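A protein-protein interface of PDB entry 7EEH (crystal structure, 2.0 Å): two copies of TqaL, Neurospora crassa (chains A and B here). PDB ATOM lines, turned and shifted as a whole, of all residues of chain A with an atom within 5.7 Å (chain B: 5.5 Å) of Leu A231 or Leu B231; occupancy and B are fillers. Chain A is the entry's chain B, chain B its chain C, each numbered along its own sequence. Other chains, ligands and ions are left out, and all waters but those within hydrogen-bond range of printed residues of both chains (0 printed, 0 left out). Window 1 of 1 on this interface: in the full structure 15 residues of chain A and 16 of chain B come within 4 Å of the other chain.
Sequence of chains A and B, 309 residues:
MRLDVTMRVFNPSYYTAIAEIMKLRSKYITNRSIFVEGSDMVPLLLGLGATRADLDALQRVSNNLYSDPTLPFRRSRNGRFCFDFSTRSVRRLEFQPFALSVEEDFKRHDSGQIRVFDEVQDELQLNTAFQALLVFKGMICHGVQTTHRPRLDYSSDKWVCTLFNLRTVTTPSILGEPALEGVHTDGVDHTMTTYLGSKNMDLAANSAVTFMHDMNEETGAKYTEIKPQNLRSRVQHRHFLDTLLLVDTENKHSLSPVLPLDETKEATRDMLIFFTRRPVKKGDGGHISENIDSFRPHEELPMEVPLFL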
ATOM      1  N   ASN A 206      -4.423   8.676  -7.009  1.00  0.00           N
ATOM      2  CA  ASN A 206      -3.232   9.499  -6.845  1.00  0.00           C
ATOM      3  C   ASN A 206      -2.265   8.751  -5.932  1.00  0.00           C
ATOM      4  O   ASN A 206      -2.030   9.092  -4.771  1.00  0.00           O
ATOM      5  CB  ASN A 206      -3.592  10.891  -6.354  1.00  0.00           C
ATOM      6  CG  ASN A 206      -3.608  11.901  -7.489  1.00  0.00           C
ATOM      7  OD1 ASN A 206      -3.900  11.541  -8.631  1.00  0.00           O
ATOM      8  ND2 ASN A 206      -3.280  13.156  -7.194  1.00  0.00           N
ATOM      9  N   VAL A 209       2.233  10.171  -6.283  1.00  0.00           N
ATOM     10  CA  VAL A 209       2.201  11.380  -7.104  1.00  0.00           C
ATOM     11  C   VAL A 209       3.150  12.400  -6.493  1.00  0.00           C
ATOM     12  O   VAL A 209       3.123  12.624  -5.278  1.00  0.00           O
ATOM     13  CB  VAL A 209       0.775  11.948  -7.208  1.00  0.00           C
ATOM     14  CG1 VAL A 209       0.796  13.368  -7.756  1.00  0.00           C
ATOM     15  CG2 VAL A 209      -0.088  11.055  -8.096  1.00  0.00           C
ATOM     16  N   PHE A 211       3.984  16.226  -6.187  1.00  0.00           N
ATOM     17  CA  PHE A 211       3.546  17.607  -6.348  1.00  0.00           C
ATOM     18  C   PHE A 211       4.744  18.529  -6.195  1.00  0.00           C
ATOM     19  O   PHE A 211       5.612  18.294  -5.357  1.00  0.00           O
ATOM     20  CB  PHE A 211       2.481  17.980  -5.311  1.00  0.00           C
ATOM     21  CG  PHE A 211       1.272  17.106  -5.357  1.00  0.00           C
ATOM     22  CD1 PHE A 211       0.246  17.379  -6.240  1.00  0.00           C
ATOM     23  CD2 PHE A 211       1.171  15.993  -4.537  1.00  0.00           C
ATOM     24  CE1 PHE A 211      -0.875  16.568  -6.306  1.00  0.00           C
ATOM     25  CE2 PHE A 211       0.049  15.168  -4.592  1.00  0.00           C
ATOM     26  CZ  PHE A 211      -0.974  15.462  -5.482  1.00  0.00           C
ATOM     27  N   MET A 212       4.791  19.579  -6.998  1.00  0.00           N
ATOM     28  CA  MET A 212       5.776  20.607  -6.738  1.00  0.00           C
ATOM     29  C   MET A 212       5.070  21.915  -6.476  1.00  0.00           C
ATOM     30  O   MET A 212       4.057  22.228  -7.108  1.00  0.00           O
ATOM     31  CB  MET A 212       6.747  20.728  -7.890  1.00  0.00           C
ATOM     32  CG  MET A 212       7.634  19.492  -8.033  1.00  0.00           C
ATOM     33  SD  MET A 212       8.390  19.607  -9.792  1.00  0.00           S
ATOM     34  CE  MET A 212       8.978  21.417  -9.649  1.00  0.00           C
ATOM     35  N   HIS A 213       5.625  22.668  -5.534  1.00  0.00           N
ATOM     36  CA  HIS A 213       4.992  23.853  -4.988  1.00  0.00           C
ATOM     37  C   HIS A 213       5.964  25.014  -5.104  1.00  0.00           C
ATOM     38  O   HIS A 213       7.181  24.821  -5.178  1.00  0.00           O
ATOM     39  CB  HIS A 213       4.588  23.644  -3.519  1.00  0.00           C
ATOM     40  CG  HIS A 213       4.125  22.254  -3.201  1.00  0.00           C
ATOM     41  ND1 HIS A 213       2.809  21.862  -3.316  1.00  0.00           N
ATOM     42  CD2 HIS A 213       4.804  21.164  -2.768  1.00  0.00           C
ATOM     43  CE1 HIS A 213       2.695  20.594  -2.964  1.00  0.00           C
ATOM     44  NE2 HIS A 213       3.893  20.145  -2.633  1.00  0.00           N
ATOM     45  N   ASP A 214       5.421  26.228  -5.136  1.00  0.00           N
ATOM     46  CA  ASP A 214       6.284  27.395  -5.046  1.00  0.00           C
ATOM     47  C   ASP A 214       6.772  27.552  -3.606  1.00  0.00           C
ATOM     48  O   ASP A 214       6.350  26.834  -2.697  1.00  0.00           O
ATOM     49  CB  ASP A 214       5.566  28.654  -5.561  1.00  0.00           C
ATOM     50  CG  ASP A 214       4.359  29.042  -4.720  1.00  0.00           C
ATOM     51  OD1 ASP A 214       4.487  29.158  -3.488  1.00  0.00           O
ATOM     52  OD2 ASP A 214       3.276  29.269  -5.299  1.00  0.00           O
ATOM     53  N   ILE A 226      -2.273  20.762   0.914  1.00  0.00           N
ATOM     54  CA  ILE A 226      -1.559  21.760   0.127  1.00  0.00           C
ATOM     55  C   ILE A 226      -2.558  22.618  -0.642  1.00  0.00           C
ATOM     56  O   ILE A 226      -3.609  22.149  -1.092  1.00  0.00           O
ATOM     57  CB  ILE A 226      -0.532  21.092  -0.808  1.00  0.00           C
ATOM     58  CG1 ILE A 226      -1.231  20.281  -1.894  1.00  0.00           C
ATOM     59  CG2 ILE A 226       0.406  20.203  -0.011  1.00  0.00           C
ATOM     60  CD1 ILE A 226      -1.219  20.956  -3.251  1.00  0.00           C
ATOM     61  N   LYS A 227      -2.225  23.890  -0.785  1.00  0.00           N
ATOM     62  CA  LYS A 227      -3.122  24.849  -1.417  1.00  0.00           C
ATOM     63  C   LYS A 227      -2.964  24.794  -2.932  1.00  0.00           C
ATOM     64  O   LYS A 227      -1.837  24.850  -3.435  1.00  0.00           O
ATOM     65  CB  LYS A 227      -2.835  26.256  -0.902  1.00  0.00           C
ATOM     66  CG  LYS A 227      -2.741  26.333   0.622  1.00  0.00           C
ATOM     67  CD  LYS A 227      -2.560  27.765   1.109  1.00  0.00           C
ATOM     68  CE  LYS A 227      -1.099  28.192   1.086  1.00  0.00           C
ATOM     69  NZ  LYS A 227      -0.392  27.957   2.380  1.00  0.00           N
ATOM     70  N   PRO A 228      -4.055  24.668  -3.688  1.00  0.00           N
ATOM     71  CA  PRO A 228      -3.925  24.679  -5.153  1.00  0.00           C
ATOM     72  C   PRO A 228      -3.288  25.951  -5.682  1.00  0.00           C
ATOM     73  O   PRO A 228      -2.606  25.915  -6.714  1.00  0.00           O
ATOM     74  CB  PRO A 228      -5.378  24.520  -5.632  1.00  0.00           C
ATOM     75  CG  PRO A 228      -6.081  23.866  -4.485  1.00  0.00           C
ATOM     76  CD  PRO A 228      -5.446  24.453  -3.255  1.00  0.00           C
ATOM     77  N   GLN A 229      -3.463  27.073  -4.982  1.00  0.00           N
ATOM     78  CA  GLN A 229      -2.886  28.339  -5.414  1.00  0.00           C
ATOM     79  C   GLN A 229      -1.364  28.301  -5.454  1.00  0.00           C
ATOM     80  O   GLN A 229      -0.748  29.134  -6.129  1.00  0.00           O
ATOM     81  CB  GLN A 229      -3.338  29.471  -4.481  1.00  0.00           C
ATOM     82  CG  GLN A 229      -4.850  29.654  -4.372  1.00  0.00           C
ATOM     83  CD  GLN A 229      -5.488  28.761  -3.306  1.00  0.00           C
ATOM     84  OE1 GLN A 229      -5.041  27.635  -3.065  1.00  0.00           O
ATOM     85  NE2 GLN A 229      -6.536  29.269  -2.663  1.00  0.00           N
ATOM     86  N   ASN A 230      -0.738  27.370  -4.738  1.00  0.00           N
ATOM     87  CA  ASN A 230       0.714  27.318  -4.660  1.00  0.00           C
ATOM     88  C   ASN A 230       1.291  26.144  -5.431  1.00  0.00           C
ATOM     89  O   ASN A 230       2.496  25.889  -5.343  1.00  0.00           O
ATOM     90  CB  ASN A 230       1.154  27.282  -3.198  1.00  0.00           C
ATOM     91  CG  ASN A 230       0.885  28.604  -2.495  1.00  0.00           C
ATOM     92  OD1 ASN A 230      -0.241  28.884  -2.104  1.00  0.00           O
ATOM     93  ND2 ASN A 230       1.905  29.438  -2.383  1.00  0.00           N
ATOM     94  N   LEU A 231       0.464  25.450  -6.204  1.00  0.00           N
ATOM     95  CA  LEU A 231       0.871  24.251  -6.918  1.00  0.00           C
ATOM     96  C   LEU A 231       1.484  24.610  -8.265  1.00  0.00           C
ATOM     97  O   LEU A 231       0.840  25.256  -9.099  1.00  0.00           O
ATOM     98  CB  LEU A 231      -0.327  23.333  -7.107  1.00  0.00           C
ATOM     99  CG  LEU A 231       0.145  21.953  -7.531  1.00  0.00           C
ATOM    100  CD1 LEU A 231       0.493  21.105  -6.330  1.00  0.00           C
ATOM    101  CD2 LEU A 231      -0.935  21.333  -8.330  1.00  0.00           C
ATOM    102  N   ARG A 232       2.724  24.180  -8.478  1.00  0.00           N
ATOM    103  CA  ARG A 232       3.442  24.440  -9.716  1.00  0.00           C
ATOM    104  C   ARG A 232       3.428  23.267 -10.687  1.00  0.00           C
ATOM    105  O   ARG A 232       3.514  23.483 -11.902  1.00  0.00           O
ATOM    106  CB  ARG A 232       4.895  24.812  -9.413  1.00  0.00           C
ATOM    107  CG  ARG A 232       5.023  26.017  -8.511  1.00  0.00           C
ATOM    108  CD  ARG A 232       5.814  27.109  -9.207  1.00  0.00           C
ATOM    109  NE  ARG A 232       7.240  26.796  -9.210  1.00  0.00           N
ATOM    110  CZ  ARG A 232       8.180  27.558  -8.653  1.00  0.00           C
ATOM    111  NH1 ARG A 232       7.856  28.703  -8.054  1.00  0.00           N
ATOM    112  NH2 ARG A 232       9.450  27.177  -8.701  1.00  0.00           N
ATOM    113  N   SER A 233       3.323  22.039 -10.189  1.00  0.00           N
ATOM    114  CA  SER A 233       3.324  20.886 -11.072  1.00  0.00           C
ATOM    115  C   SER A 233       2.777  19.687 -10.322  1.00  0.00           C
ATOM    116  O   SER A 233       2.881  19.610  -9.098  1.00  0.00           O
ATOM    117  CB  SER A 233       4.735  20.588 -11.589  1.00  0.00           C
ATOM    118  OG  SER A 233       4.664  19.739 -12.713  1.00  0.00           O
ATOM    119  N   ARG A 234       2.195  18.755 -11.079  1.00  0.00           N
ATOM    120  CA  ARG A 234       1.748  17.465 -10.575  1.00  0.00           C
ATOM    121  C   ARG A 234       2.247  16.403 -11.541  1.00  0.00           C
ATOM    122  O   ARG A 234       2.015  16.500 -12.749  1.00  0.00           O
ATOM    123  CB  ARG A 234       0.218  17.405 -10.447  1.00  0.00           C
ATOM    124  CG  ARG A 234      -0.356  16.077  -9.930  1.00  0.00           C
ATOM    125  CD  ARG A 234      -0.567  15.049 -11.065  1.00  0.00           C
ATOM    126  NE  ARG A 234      -1.405  13.929 -10.664  1.00  0.00           N
ATOM    127  CZ  ARG A 234      -1.489  12.781 -11.336  1.00  0.00           C
ATOM    128  NH1 ARG A 234      -0.779  12.597 -12.444  1.00  0.00           N
ATOM    129  NH2 ARG A 234      -2.283  11.813 -10.902  1.00  0.00           N
ATOM    130  N   ASN B 206      -0.471  31.668  -9.270  1.00  0.00           N
ATOM    131  CA  ASN B 206      -1.213  30.743 -10.121  1.00  0.00           C
ATOM    132  C   ASN B 206      -2.230  31.545 -10.932  1.00  0.00           C
ATOM    133  O   ASN B 206      -3.448  31.501 -10.733  1.00  0.00           O
ATOM    134  CB  ASN B 206      -1.822  29.626  -9.294  1.00  0.00           C
ATOM    135  CG  ASN B 206      -0.938  28.388  -9.296  1.00  0.00           C
ATOM    136  OD1 ASN B 206       0.250  28.470  -9.635  1.00  0.00           O
ATOM    137  ND2 ASN B 206      -1.507  27.240  -8.933  1.00  0.00           N
ATOM    138  N   VAL B 209      -4.069  29.325 -14.461  1.00  0.00           N
ATOM    139  CA  VAL B 209      -3.567  27.952 -14.434  1.00  0.00           C
ATOM    140  C   VAL B 209      -4.711  27.015 -14.793  1.00  0.00           C
ATOM    141  O   VAL B 209      -5.827  27.162 -14.276  1.00  0.00           O
ATOM    142  CB  VAL B 209      -2.985  27.604 -13.051  1.00  0.00           C
ATOM    143  CG1 VAL B 209      -2.721  26.121 -12.936  1.00  0.00           C
ATOM    144  CG2 VAL B 209      -1.693  28.381 -12.791  1.00  0.00           C
ATOM    145  N   PHE B 211      -6.148  23.368 -14.378  1.00  0.00           N
ATOM    146  CA  PHE B 211      -6.067  22.132 -13.615  1.00  0.00           C
ATOM    147  C   PHE B 211      -6.872  21.071 -14.334  1.00  0.00           C
ATOM    148  O   PHE B 211      -7.928  21.356 -14.901  1.00  0.00           O
ATOM    149  CB  PHE B 211      -6.597  22.292 -12.185  1.00  0.00           C
ATOM    150  CG  PHE B 211      -5.903  23.358 -11.400  1.00  0.00           C
ATOM    151  CD1 PHE B 211      -4.779  23.061 -10.650  1.00  0.00           C
ATOM    152  CD2 PHE B 211      -6.369  24.673 -11.427  1.00  0.00           C
ATOM    153  CE1 PHE B 211      -4.129  24.057  -9.928  1.00  0.00           C
ATOM    154  CE2 PHE B 211      -5.724  25.679 -10.709  1.00  0.00           C
ATOM    155  CZ  PHE B 211      -4.605  25.369  -9.958  1.00  0.00           C
ATOM    156  N   MET B 212      -6.361  19.853 -14.319  1.00  0.00           N
ATOM    157  CA  MET B 212      -7.148  18.736 -14.790  1.00  0.00           C
ATOM    158  C   MET B 212      -7.378  17.740 -13.680  1.00  0.00           C
ATOM    159  O   MET B 212      -6.474  17.450 -12.884  1.00  0.00           O
ATOM    160  CB  MET B 212      -6.478  18.065 -15.965  1.00  0.00           C
ATOM    161  CG  MET B 212      -6.918  18.649 -17.292  1.00  0.00           C
ATOM    162  SD  MET B 212      -5.739  17.898 -18.597  1.00  0.00           S
ATOM    163  CE  MET B 212      -4.336  19.142 -18.409  1.00  0.00           C
ATOM    164  N   HIS B 213      -8.592  17.205 -13.666  1.00  0.00           N
ATOM    165  CA  HIS B 213      -9.113  16.418 -12.565  1.00  0.00           C
ATOM    166  C   HIS B 213      -9.643  15.103 -13.105  1.00  0.00           C
ATOM    167  O   HIS B 213     -10.080  15.023 -14.253  1.00  0.00           O
ATOM    168  CB  HIS B 213     -10.239  17.173 -11.833  1.00  0.00           C
ATOM    169  CG  HIS B 213      -9.971  18.634 -11.648  1.00  0.00           C
ATOM    170  ND1 HIS B 213      -9.232  19.127 -10.593  1.00  0.00           N
ATOM    171  CD2 HIS B 213     -10.346  19.711 -12.383  1.00  0.00           C
ATOM    172  CE1 HIS B 213      -9.172  20.445 -10.681  1.00  0.00           C
ATOM    173  NE2 HIS B 213      -9.829  20.824 -11.766  1.00  0.00           N
ATOM    174  N   ASP B 214      -9.603  14.070 -12.273  1.00  0.00           N
ATOM    175  CA  ASP B 214     -10.265  12.832 -12.651  1.00  0.00           C
ATOM    176  C   ASP B 214     -11.783  12.993 -12.527  1.00  0.00           C
ATOM    177  O   ASP B 214     -12.284  13.985 -11.975  1.00  0.00           O
ATOM    178  CB  ASP B 214      -9.745  11.653 -11.813  1.00  0.00           C
ATOM    179  CG  ASP B 214     -10.106  11.751 -10.332  1.00  0.00           C
ATOM    180  OD1 ASP B 214     -11.245  12.114  -9.985  1.00  0.00           O
ATOM    181  OD2 ASP B 214      -9.239  11.425  -9.498  1.00  0.00           O
ATOM    182  N   ILE B 226     -10.502  22.341  -4.915  1.00  0.00           N
ATOM    183  CA  ILE B 226     -10.290  21.026  -5.512  1.00  0.00           C
ATOM    184  C   ILE B 226      -9.366  20.206  -4.621  1.00  0.00           C
ATOM    185  O   ILE B 226      -8.473  20.732  -3.947  1.00  0.00           O
ATOM    186  CB  ILE B 226      -9.732  21.142  -6.943  1.00  0.00           C
ATOM    187  CG1 ILE B 226      -8.314  21.721  -6.926  1.00  0.00           C
ATOM    188  CG2 ILE B 226     -10.682  21.953  -7.816  1.00  0.00           C
ATOM    189  CD1 ILE B 226      -7.230  20.688  -7.204  1.00  0.00           C
ATOM    190  N   LYS B 227      -9.583  18.895  -4.629  1.00  0.00           N
ATOM    191  CA  LYS B 227      -8.804  17.980  -3.805  1.00  0.00           C
ATOM    192  C   LYS B 227      -7.544  17.553  -4.546  1.00  0.00           C
ATOM    193  O   LYS B 227      -7.643  17.062  -5.682  1.00  0.00           O
ATOM    194  CB  LYS B 227      -9.629  16.753  -3.428  1.00  0.00           C
ATOM    195  CG  LYS B 227     -10.986  17.062  -2.799  1.00  0.00           C
ATOM    196  CD  LYS B 227     -11.910  15.844  -2.855  1.00  0.00           C
ATOM    197  CE  LYS B 227     -12.765  15.842  -4.127  1.00  0.00           C
ATOM    198  NZ  LYS B 227     -13.723  14.696  -4.198  1.00  0.00           N
ATOM    199  N   PRO B 228      -6.361  17.732  -3.963  1.00  0.00           N
ATOM    200  CA  PRO B 228      -5.129  17.220  -4.592  1.00  0.00           C
ATOM    201  C   PRO B 228      -5.186  15.757  -5.015  1.00  0.00           C
ATOM    202  O   PRO B 228      -4.585  15.394  -6.033  1.00  0.00           O
ATOM    203  CB  PRO B 228      -4.068  17.439  -3.502  1.00  0.00           C
ATOM    204  CG  PRO B 228      -4.650  18.439  -2.546  1.00  0.00           C
ATOM    205  CD  PRO B 228      -6.085  18.706  -2.898  1.00  0.00           C
ATOM    206  N   GLN B 229      -5.891  14.901  -4.277  1.00  0.00           N
ATOM    207  CA  GLN B 229      -5.923  13.480  -4.606  1.00  0.00           C
ATOM    208  C   GLN B 229      -6.683  13.185  -5.896  1.00  0.00           C
ATOM    209  O   GLN B 229      -6.575  12.068  -6.416  1.00  0.00           O
ATOM    210  CB  GLN B 229      -6.533  12.672  -3.448  1.00  0.00           C
ATOM    211  CG  GLN B 229      -7.754  13.309  -2.788  1.00  0.00           C
ATOM    212  CD  GLN B 229      -7.393  14.398  -1.779  1.00  0.00           C
ATOM    213  OE1 GLN B 229      -7.124  15.549  -2.149  1.00  0.00           O
ATOM    214  NE2 GLN B 229      -7.373  14.035  -0.502  1.00  0.00           N
ATOM    215  N   ASN B 230      -7.446  14.143  -6.418  1.00  0.00           N
ATOM    216  CA  ASN B 230      -8.134  13.982  -7.691  1.00  0.00           C
ATOM    217  C   ASN B 230      -7.479  14.782  -8.807  1.00  0.00           C
ATOM    218  O   ASN B 230      -8.004  14.817  -9.924  1.00  0.00           O
ATOM    219  CB  ASN B 230      -9.605  14.371  -7.545  1.00  0.00           C
ATOM    220  CG  ASN B 230     -10.340  13.451  -6.592  1.00  0.00           C
ATOM    221  OD1 ASN B 230     -10.382  13.696  -5.391  1.00  0.00           O
ATOM    222  ND2 ASN B 230     -10.891  12.370  -7.117  1.00  0.00           N
ATOM    223  N   LEU B 231      -6.345  15.413  -8.527  1.00  0.00           N
ATOM    224  CA  LEU B 231      -5.659  16.234  -9.511  1.00  0.00           C
ATOM    225  C   LEU B 231      -4.826  15.377 -10.460  1.00  0.00           C
ATOM    226  O   LEU B 231      -3.991  14.578 -10.022  1.00  0.00           O
ATOM    227  CB  LEU B 231      -4.780  17.242  -8.790  1.00  0.00           C
ATOM    228  CG  LEU B 231      -4.210  18.372  -9.620  1.00  0.00           C
ATOM    229  CD1 LEU B 231      -5.310  19.264 -10.195  1.00  0.00           C
ATOM    230  CD2 LEU B 231      -3.355  19.126  -8.677  1.00  0.00           C
ATOM    231  N   ARG B 232      -5.051  15.543 -11.763  1.00  0.00           N
ATOM    232  CA  ARG B 232      -4.307  14.776 -12.753  1.00  0.00           C
ATOM    233  C   ARG B 232      -3.208  15.571 -13.459  1.00  0.00           C
ATOM    234  O   ARG B 232      -2.214  14.978 -13.878  1.00  0.00           O
ATOM    235  CB  ARG B 232      -5.256  14.176 -13.796  1.00  0.00           C
ATOM    236  CG  ARG B 232      -5.860  12.879 -13.308  1.00  0.00           C
ATOM    237  CD  ARG B 232      -6.272  11.935 -14.430  1.00  0.00           C
ATOM    238  NE  ARG B 232      -7.185  10.892 -13.942  1.00  0.00           N
ATOM    239  CZ  ARG B 232      -6.881   9.968 -13.021  1.00  0.00           C
ATOM    240  NH1 ARG B 232      -5.666   9.916 -12.473  1.00  0.00           N
ATOM    241  NH2 ARG B 232      -7.798   9.073 -12.655  1.00  0.00           N
ATOM    242  N   SER B 233      -3.351  16.886 -13.600  1.00  0.00           N
ATOM    243  CA  SER B 233      -2.189  17.692 -13.945  1.00  0.00           C
ATOM    244  C   SER B 233      -2.502  19.150 -13.670  1.00  0.00           C
ATOM    245  O   SER B 233      -3.638  19.522 -13.360  1.00  0.00           O
ATOM    246  CB  SER B 233      -1.764  17.517 -15.400  1.00  0.00           C
ATOM    247  OG  SER B 233      -2.769  18.005 -16.240  1.00  0.00           O
ATOM    248  N   ARG B 234      -1.458  19.963 -13.787  1.00  0.00           N
ATOM    249  CA  ARG B 234      -1.515  21.403 -13.617  1.00  0.00           C
ATOM    250  C   ARG B 234      -0.601  22.000 -14.673  1.00  0.00           C
ATOM    251  O   ARG B 234       0.584  21.652 -14.730  1.00  0.00           O
ATOM    252  CB  ARG B 234      -1.061  21.795 -12.205  1.00  0.00           C
ATOM    253  CG  ARG B 234      -0.963  23.297 -11.931  1.00  0.00           C
ATOM    254  CD  ARG B 234       0.398  23.859 -12.316  1.00  0.00           C
ATOM    255  NE  ARG B 234       0.589  25.247 -11.907  1.00  0.00           N
ATOM    256  CZ  ARG B 234       1.431  26.080 -12.510  1.00  0.00           C
ATOM    257  NH1 ARG B 234       2.139  25.661 -13.551  1.00  0.00           N
ATOM    258  NH2 ARG B 234       1.562  27.329 -12.076  1.00  0.00           N
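The side-chain amide nitrogen (ND2) of Asn A206 is in hydrogen-bond range of the backbone carbonyl oxygen (O) of Pro B228 (2.8 Å).
ND2 of Asn A206 sits at hydrogen-bond distance from O of Leu B231.
The backbone carbonyl oxygen (O) of Pro A228 sits at hydrogen-bond distance from the side-chain amide nitrogen (ND2) of Asn B206.
The backbone carbonyl oxygen (O) of Gln A229 lies close to the side-chain amide nitrogen (ND2) of Asn B206 (3.5 Å).
The backbone carbonyl oxygen (O) of Leu A231 is in hydrogen-bond range of the side-chain amide nitrogen (ND2) of Asn B206, at 3.1 Å.
The backbone carbonyl oxygen (O) of Leu A231 lies within hydrogen-bond range of the guanidinium group (NE) of Arg B234, at 2.8 Å.
The backbone carbonyl oxygen of Arg A232 sits at hydrogen-bond distance from the guanidinium group of Arg B234 (3.1 Å).
The backbone carbonyl oxygen (O) of Leu B231 is in hydrogen-bond range of the guanidinium group (NE) of Arg A234 (2.7 Å).
NH1 of Arg A234 lies within hydrogen-bond range of O of Arg B232.
Asn A206 touches Gln B229 (CG to O, 3.2 Å).
O of Pro B228 touches CZ of Phe A211, 3.7 Å away.
Ile A226 touches Pro B228.
Pro A228 touches Phe B211.
Pro A228 touches Ile B226 (CG to CG1, 3.9 Å).
Leu B231 touches Leu A231 (CD2 to CD2, 3.3 Å).
Asn A206 touches Gln B229, and with the chains exchanged Gln A229 touches Asn B206.
Leu A231 touches its own counterpart, Leu B231.
Leu A231 touches Arg B234, and with the chains exchanged Arg A234 touches Leu B231.
Arg A232 touches Arg B234, and with the chains exchanged Arg A234 touches Arg B232.
Of the 15 printed residues of chain A, 8 touch a printed residue of chain B.
Of the 15 printed residues of chain B, 8 touch a printed residue of chain A.
Of chain B, only Asn B206, Leu B231 and Arg B234 come within 4 Å of Leu A231.
Printed residues of chain A within 4 Å of Leu B231: Asn A206, Leu A231 and Arg A234.
Printed residues of chain B within 4 Å of Gln A229: Asn B206 (3.3 Å).
Of the printed residues of chain B, Arg A232 touches Arg B234 (3.1 Å).
Printed residues of chain A within 4 Å of Ile B226: Pro A228 (3.9 Å).
His A213 touches none of the printed residues of chain B.
The nearest printed residue of chain A that does not touch Leu B231 is Phe A211 (4.3 Å).
The nearest printed residue of chain A that does not touch Ile B226 is Ile A226 (5.8 Å).
The side-chain amide oxygen (OD1) of Asn A206 is in hydrogen-bond range of the guanidinium group (NH2) of Arg A234.
O of Met A212 sits at hydrogen-bond distance from N of Arg A232 (2.7 Å).
OD1 of Asn B206 is in hydrogen-bond range of NH2 of Arg B234 (3.0 Å).
The backbone NH of Arg B232 lies within hydrogen-bond range of the backbone carbonyl oxygen of Met B212 (2.6 Å).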
